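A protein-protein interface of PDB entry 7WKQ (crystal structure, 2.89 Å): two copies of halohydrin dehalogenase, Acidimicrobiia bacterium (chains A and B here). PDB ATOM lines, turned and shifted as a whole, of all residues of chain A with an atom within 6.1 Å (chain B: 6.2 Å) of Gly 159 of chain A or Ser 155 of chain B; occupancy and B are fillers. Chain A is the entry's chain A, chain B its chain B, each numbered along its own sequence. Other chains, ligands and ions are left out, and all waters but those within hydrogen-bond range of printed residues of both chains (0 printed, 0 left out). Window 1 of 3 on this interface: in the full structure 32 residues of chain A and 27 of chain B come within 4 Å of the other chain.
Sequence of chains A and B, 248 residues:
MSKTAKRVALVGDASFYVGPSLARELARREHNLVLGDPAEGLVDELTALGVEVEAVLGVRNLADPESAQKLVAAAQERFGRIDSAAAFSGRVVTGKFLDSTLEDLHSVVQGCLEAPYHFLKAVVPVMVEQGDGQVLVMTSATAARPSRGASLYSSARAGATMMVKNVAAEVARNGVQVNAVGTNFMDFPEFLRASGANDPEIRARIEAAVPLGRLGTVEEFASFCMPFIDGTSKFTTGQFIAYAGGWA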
ATOM      1  N   LEU A 113      17.340 -10.247  17.774  1.00  0.00           N
ATOM      2  CA  LEU A 113      16.652 -10.060  19.074  1.00  0.00           C
ATOM      3  C   LEU A 113      17.477 -10.643  20.230  1.00  0.00           C
ATOM      4  O   LEU A 113      17.746  -9.911  21.181  1.00  0.00           O
ATOM      5  CB  LEU A 113      15.283 -10.732  18.950  1.00  0.00           C
ATOM      6  CG  LEU A 113      14.140 -10.133  19.757  1.00  0.00           C
ATOM      7  CD1 LEU A 113      14.152  -8.626  19.653  1.00  0.00           C
ATOM      8  CD2 LEU A 113      12.812 -10.678  19.270  1.00  0.00           C
ATOM      9  N   SER A 154      12.233  -8.064   8.848  1.00  0.00           N
ATOM     10  CA  SER A 154      11.648  -6.810   9.310  1.00  0.00           C
ATOM     11  C   SER A 154      10.890  -6.987  10.628  1.00  0.00           C
ATOM     12  O   SER A 154      10.899  -6.083  11.478  1.00  0.00           O
ATOM     13  CB  SER A 154      10.754  -6.207   8.239  1.00  0.00           C
ATOM     14  OG  SER A 154      10.518  -4.849   8.559  1.00  0.00           O
ATOM     15  N   SER A 155      10.167  -8.101  10.785  1.00  0.00           N
ATOM     16  CA  SER A 155       9.454  -8.332  12.043  1.00  0.00           C
ATOM     17  C   SER A 155      10.427  -8.405  13.225  1.00  0.00           C
ATOM     18  O   SER A 155      10.232  -7.748  14.267  1.00  0.00           O
ATOM     19  CB  SER A 155       8.622  -9.601  11.947  1.00  0.00           C
ATOM     20  OG  SER A 155       7.849  -9.582  10.763  1.00  0.00           O
ATOM     21  N   ALA A 156      11.475  -9.223  13.086  1.00  0.00           N
ATOM     22  CA  ALA A 156      12.487  -9.295  14.140  1.00  0.00           C
ATOM     23  C   ALA A 156      13.184  -7.950  14.341  1.00  0.00           C
ATOM     24  O   ALA A 156      13.438  -7.549  15.482  1.00  0.00           O
ATOM     25  CB  ALA A 156      13.525 -10.372  13.835  1.00  0.00           C
ATOM     26  N   ARG A 157      13.436  -7.207  13.259  1.00  0.00           N
ATOM     27  CA  ARG A 157      14.169  -5.955  13.367  1.00  0.00           C
ATOM     28  C   ARG A 157      13.307  -4.904  14.081  1.00  0.00           C
ATOM     29  O   ARG A 157      13.790  -4.195  14.984  1.00  0.00           O
ATOM     30  CB  ARG A 157      14.628  -5.558  11.962  1.00  0.00           C
ATOM     31  CG  ARG A 157      15.753  -4.525  11.784  1.00  0.00           C
ATOM     32  CD  ARG A 157      17.122  -4.889  12.260  1.00  0.00           C
ATOM     33  NE  ARG A 157      17.287  -4.280  13.564  1.00  0.00           N
ATOM     34  CZ  ARG A 157      18.109  -4.713  14.510  1.00  0.00           C
ATOM     35  NH1 ARG A 157      18.906  -5.767  14.308  1.00  0.00           N
ATOM     36  NH2 ARG A 157      18.124  -4.072  15.668  1.00  0.00           N
ATOM     37  N   ALA A 158      11.995  -4.900  13.802  1.00  0.00           N
ATOM     38  CA  ALA A 158      11.069  -4.060  14.554  1.00  0.00           C
ATOM     39  C   ALA A 158      11.045  -4.426  16.029  1.00  0.00           C
ATOM     40  O   ALA A 158      11.135  -3.545  16.902  1.00  0.00           O
ATOM     41  CB  ALA A 158       9.662  -4.192  13.999  1.00  0.00           C
ATOM     42  N   GLY A 159      10.890  -5.724  16.324  1.00  0.00           N
ATOM     43  CA  GLY A 159      10.854  -6.156  17.710  1.00  0.00           C
ATOM     44  C   GLY A 159      12.106  -5.742  18.444  1.00  0.00           C
ATOM     45  O   GLY A 159      12.048  -5.303  19.600  1.00  0.00           O
ATOM     46  N   ALA A 160      13.252  -5.782  17.751  1.00  0.00           N
ATOM     47  CA  ALA A 160      14.497  -5.397  18.407  1.00  0.00           C
ATOM     48  C   ALA A 160      14.542  -3.890  18.663  1.00  0.00           C
ATOM     49  O   ALA A 160      15.024  -3.448  19.725  1.00  0.00           O
ATOM     50  CB  ALA A 160      15.685  -5.841  17.565  1.00  0.00           C
ATOM     51  N   THR A 161      14.004  -3.098  17.729  1.00  0.00           N
ATOM     52  CA  THR A 161      13.928  -1.659  17.952  1.00  0.00           C
ATOM     53  C   THR A 161      13.140  -1.362  19.222  1.00  0.00           C
ATOM     54  O   THR A 161      13.600  -0.611  20.103  1.00  0.00           O
ATOM     55  CB  THR A 161      13.338  -0.959  16.730  1.00  0.00           C
ATOM     56  OG1 THR A 161      14.249  -1.138  15.653  1.00  0.00           O
ATOM     57  CG2 THR A 161      13.194   0.531  16.939  1.00  0.00           C
ATOM     58  N   MET A 162      11.913  -1.877  19.276  1.00  0.00           N
ATOM     59  CA  MET A 162      11.085  -1.742  20.465  1.00  0.00           C
ATOM     60  C   MET A 162      11.824  -2.157  21.745  1.00  0.00           C
ATOM     61  O   MET A 162      11.777  -1.431  22.744  1.00  0.00           O
ATOM     62  CB  MET A 162       9.804  -2.527  20.255  1.00  0.00           C
ATOM     63  CG  MET A 162       8.739  -2.387  21.300  1.00  0.00           C
ATOM     64  SD  MET A 162       8.256  -0.651  21.510  1.00  0.00           S
ATOM     65  CE  MET A 162       7.656  -0.266  19.872  1.00  0.00           C
ATOM     66  N   MET A 163      12.486  -3.325  21.751  1.00  0.00           N
ATOM     67  CA  MET A 163      13.257  -3.758  22.926  1.00  0.00           C
ATOM     68  C   MET A 163      14.283  -2.705  23.354  1.00  0.00           C
ATOM     69  O   MET A 163      14.349  -2.322  24.528  1.00  0.00           O
ATOM     70  CB  MET A 163      13.972  -5.077  22.631  1.00  0.00           C
ATOM     71  CG  MET A 163      14.732  -5.671  23.810  1.00  0.00           C
ATOM     72  SD  MET A 163      15.650  -7.138  23.289  1.00  0.00           S
ATOM     73  CE  MET A 163      14.347  -8.378  23.252  1.00  0.00           C
ATOM     74  N   VAL A 164      15.131  -2.257  22.421  1.00  0.00           N
ATOM     75  CA  VAL A 164      16.174  -1.291  22.776  1.00  0.00           C
ATOM     76  C   VAL A 164      15.564   0.016  23.285  1.00  0.00           C
ATOM     77  O   VAL A 164      16.053   0.598  24.261  1.00  0.00           O
ATOM     78  CB  VAL A 164      17.108  -1.047  21.574  1.00  0.00           C
ATOM     79  CG1 VAL A 164      17.842   0.273  21.735  1.00  0.00           C
ATOM     80  CG2 VAL A 164      18.085  -2.200  21.430  1.00  0.00           C
ATOM     81  N   ASN A 166      12.644   0.354  24.859  1.00  0.00           N
ATOM     82  CA  ASN A 166      12.189   0.043  26.203  1.00  0.00           C
ATOM     83  C   ASN A 166      13.349   0.058  27.199  1.00  0.00           C
ATOM     84  O   ASN A 166      13.219   0.574  28.328  1.00  0.00           O
ATOM     85  CB  ASN A 166      11.511  -1.333  26.227  1.00  0.00           C
ATOM     86  CG  ASN A 166      10.053  -1.283  25.819  1.00  0.00           C
ATOM     87  OD1 ASN A 166       9.229  -0.637  26.474  1.00  0.00           O
ATOM     88  ND2 ASN A 166       9.717  -1.984  24.742  1.00  0.00           N
ATOM     89  N   ALA B 150       6.530  -4.158  30.406  1.00  0.00           N
ATOM     90  CA  ALA B 150       6.568  -5.468  29.718  1.00  0.00           C
ATOM     91  C   ALA B 150       7.485  -5.348  28.509  1.00  0.00           C
ATOM     92  O   ALA B 150       6.992  -5.533  27.397  1.00  0.00           O
ATOM     93  CB  ALA B 150       5.181  -5.854  29.290  1.00  0.00           C
ATOM     94  N   SER B 151       8.768  -5.082  28.729  1.00  0.00           N
ATOM     95  CA  SER B 151       9.667  -4.831  27.602  1.00  0.00           C
ATOM     96  C   SER B 151       9.567  -5.916  26.543  1.00  0.00           C
ATOM     97  O   SER B 151       9.299  -5.629  25.364  1.00  0.00           O
ATOM     98  CB  SER B 151      11.113  -4.757  28.072  1.00  0.00           C
ATOM     99  OG  SER B 151      11.333  -3.697  28.972  1.00  0.00           O
ATOM    100  N   LEU B 152       9.746  -7.180  26.952  1.00  0.00           N
ATOM    101  CA  LEU B 152       9.858  -8.245  25.966  1.00  0.00           C
ATOM    102  C   LEU B 152       8.538  -8.437  25.218  1.00  0.00           C
ATOM    103  O   LEU B 152       8.523  -8.619  23.992  1.00  0.00           O
ATOM    104  CB  LEU B 152      10.347  -9.542  26.629  1.00  0.00           C
ATOM    105  CG  LEU B 152      11.727  -9.482  27.324  1.00  0.00           C
ATOM    106  CD1 LEU B 152      12.194 -10.898  27.795  1.00  0.00           C
ATOM    107  CD2 LEU B 152      12.799  -8.684  26.572  1.00  0.00           C
ATOM    108  N   TYR B 153       7.429  -8.441  25.948  1.00  0.00           N
ATOM    109  CA  TYR B 153       6.116  -8.548  25.328  1.00  0.00           C
ATOM    110  C   TYR B 153       5.855  -7.429  24.317  1.00  0.00           C
ATOM    111  O   TYR B 153       5.411  -7.680  23.182  1.00  0.00           O
ATOM    112  CB  TYR B 153       5.054  -8.529  26.403  1.00  0.00           C
ATOM    113  CG  TYR B 153       3.759  -8.945  25.838  1.00  0.00           C
ATOM    114  CD1 TYR B 153       3.585 -10.253  25.416  1.00  0.00           C
ATOM    115  CD2 TYR B 153       2.722  -8.034  25.673  1.00  0.00           C
ATOM    116  CE1 TYR B 153       2.407 -10.663  24.887  1.00  0.00           C
ATOM    117  CE2 TYR B 153       1.522  -8.430  25.135  1.00  0.00           C
ATOM    118  CZ  TYR B 153       1.376  -9.749  24.737  1.00  0.00           C
ATOM    119  OH  TYR B 153       0.193 -10.172  24.193  1.00  0.00           O
ATOM    120  N   SER B 154       6.049  -6.193  24.740  1.00  0.00           N
ATOM    121  CA  SER B 154       5.848  -5.063  23.812  1.00  0.00           C
ATOM    122  C   SER B 154       6.668  -5.327  22.560  1.00  0.00           C
ATOM    123  O   SER B 154       6.194  -5.011  21.465  1.00  0.00           O
ATOM    124  CB  SER B 154       6.271  -3.792  24.455  1.00  0.00           C
ATOM    125  OG  SER B 154       6.121  -2.703  23.562  1.00  0.00           O
ATOM    126  N   SER B 155       7.858  -5.886  22.729  1.00  0.00           N
ATOM    127  CA  SER B 155       8.757  -6.108  21.576  1.00  0.00           C
ATOM    128  C   SER B 155       8.167  -7.102  20.577  1.00  0.00           C
ATOM    129  O   SER B 155       8.208  -6.825  19.377  1.00  0.00           O
ATOM    130  CB  SER B 155      10.081  -6.565  22.072  1.00  0.00           C
ATOM    131  OG  SER B 155      10.589  -5.654  23.029  1.00  0.00           O
ATOM    132  N   ALA B 156       7.621  -8.211  21.054  1.00  0.00           N
ATOM    133  CA  ALA B 156       7.070  -9.251  20.163  1.00  0.00           C
ATOM    134  C   ALA B 156       5.847  -8.734  19.422  1.00  0.00           C
ATOM    135  O   ALA B 156       5.638  -9.133  18.281  1.00  0.00           O
ATOM    136  CB  ALA B 156       6.740 -10.457  20.970  1.00  0.00           C
ATOM    137  N   ARG B 157       5.042  -7.922  20.086  1.00  0.00           N
ATOM    138  CA  ARG B 157       3.817  -7.381  19.459  1.00  0.00           C
ATOM    139  C   ARG B 157       4.241  -6.533  18.276  1.00  0.00           C
ATOM    140  O   ARG B 157       3.581  -6.573  17.246  1.00  0.00           O
ATOM    141  CB  ARG B 157       3.091  -6.497  20.474  1.00  0.00           C
ATOM    142  CG  ARG B 157       1.606  -6.305  20.210  1.00  0.00           C
ATOM    143  CD  ARG B 157       1.156  -4.921  20.636  1.00  0.00           C
ATOM    144  NE  ARG B 157       2.196  -3.925  20.440  1.00  0.00           N
ATOM    145  CZ  ARG B 157       2.281  -3.118  19.390  1.00  0.00           C
ATOM    146  NH1 ARG B 157       3.271  -2.246  19.304  1.00  0.00           N
ATOM    147  NH2 ARG B 157       1.381  -3.185  18.426  1.00  0.00           N
ATOM    148  N   ALA B 158       5.312  -5.784  18.453  1.00  0.00           N
ATOM    149  CA  ALA B 158       5.791  -4.907  17.377  1.00  0.00           C
ATOM    150  C   ALA B 158       6.181  -5.762  16.183  1.00  0.00           C
ATOM    151  O   ALA B 158       5.886  -5.371  15.054  1.00  0.00           O
ATOM    152  CB  ALA B 158       6.965  -4.147  17.898  1.00  0.00           C
ATOM    153  N   GLY B 159       6.848  -6.874  16.442  1.00  0.00           N
ATOM    154  CA  GLY B 159       7.220  -7.783  15.354  1.00  0.00           C
ATOM    155  C   GLY B 159       5.990  -8.363  14.719  1.00  0.00           C
ATOM    156  O   GLY B 159       5.952  -8.470  13.501  1.00  0.00           O
ATOM    157  N   ALA B 160       5.017  -8.726  15.536  1.00  0.00           N
ATOM    158  CA  ALA B 160       3.797  -9.343  14.999  1.00  0.00           C
ATOM    159  C   ALA B 160       3.068  -8.273  14.212  1.00  0.00           C
ATOM    160  O   ALA B 160       2.485  -8.591  13.178  1.00  0.00           O
ATOM    161  CB  ALA B 160       2.971  -9.869  16.124  1.00  0.00           C
ATOM    162  N   MET B 162       4.582  -5.679  12.527  1.00  0.00           N
ATOM    163  CA  MET B 162       5.298  -5.770  11.243  1.00  0.00           C
ATOM    164  C   MET B 162       4.919  -6.970  10.416  1.00  0.00           C
ATOM    165  O   MET B 162       4.803  -6.855   9.194  1.00  0.00           O
ATOM    166  CB  MET B 162       6.803  -5.878  11.378  1.00  0.00           C
ATOM    167  CG  MET B 162       7.481  -4.550  11.634  1.00  0.00           C
ATOM    168  SD  MET B 162       7.203  -3.431  10.222  1.00  0.00           S
ATOM    169  CE  MET B 162       6.092  -2.316  11.142  1.00  0.00           C
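Gly 159 of chain A touches one residue of chain B. Val 164 of chain A touches none of the printed residues of chain B. Printed residues of chain B within 4 Å of Asn 166 of chain A: Ser 151 (3.6 Å) and Ser 154 (3.9 Å). Printed residues of chain A within 4 Å of Ser 151 of chain B: Asn 166. Of the printed residues of chain A, Leu 152 of chain B touches Met 163. Ala 158 of chain B touches none of the printed residues of chain A. Of the printed residues of chain A, Gly 159 of chain B touches Ser 155.
Among the printed residues, pairs that only touch across the chains: Gly 159 of chain A with Ser 155 of chain B, Ser 155 of chain A with Gly 159 of chain B, Ala 158 of chain A with Met 162 of chain B, Asn 166 of chain A with Ser 151 of chain B, Ser 155 of chain A with Met 162 of chain B, Met 163 of chain A with Leu 152 of chain B, Met 162 of chain A with Ser 155 of chain B, Ser 154 of chain A with Met 162 of chain B and Asn 166 of chain A with Ser 154 of chain B.
Ser 154 of chain A touches Met 162 of chain B, and with the chains exchanged Met 162 of chain A touches Ser 154 of chain B. Ser 155 of chain A touches Gly 159 of chain B, and with the chains exchanged Gly 159 of chain A touches Ser 155 of chain B. Ser 155 of chain A touches Met 162 of chain B, and with the chains exchanged Met 162 of chain A touches Ser 155 of chain B. Ala 158 of chain A touches Met 162 of chain B, but with the chains exchanged Met 162 of chain A does not touch Ala 158 of chain B (4.03 Å). Positions printed for both chains: 154, 155, 156, 157, 158, 159, 160 and 162.
The side-chain sulfur (SD) of Met 162 of chain A sits close to the side-chain hydroxyl (OG) of Ser 154 of chain B, at 3.6 Å. N of Met 163 of chain A is in hydrogen-bond range of OG of Ser 155 of chain B, 3.3 Å away.
The backbone carbonyl oxygen (O) of Met 162 of chain A is in hydrogen-bond range of the side-chain amide nitrogen (ND2) of Asn 166 of chain A (2.9 Å). The side-chain hydroxyl (OG) of Ser 155 of chain B sits at hydrogen-bond distance from the backbone carbonyl oxygen (O) of Ser 151 of chain B, at 2.7 Å.
Of the 13 printed residues of chain A, 7 touch a printed residue of chain B. Printed residues of chain A that touch a printed residue of chain B: Ser 154, Ser 155, Ala 158, Gly 159, Met 162, Met 163 and Asn 166. Hydrophobic or aromatic side chains of chain A that line the printed part of chain B: Ala 158, Met 162 and Met 163. Of the 12 printed residues of chain B, 6 touch a printed residue of chain A. Hydrophobic or aromatic side chains of chain B within 4 Å of the printed part of chain A: Leu 152 and Met 162. Among the printed residues, no Asp or Glu carboxylate lies within 4 Å of a Lys or Arg side-chain nitrogen of the other chain.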
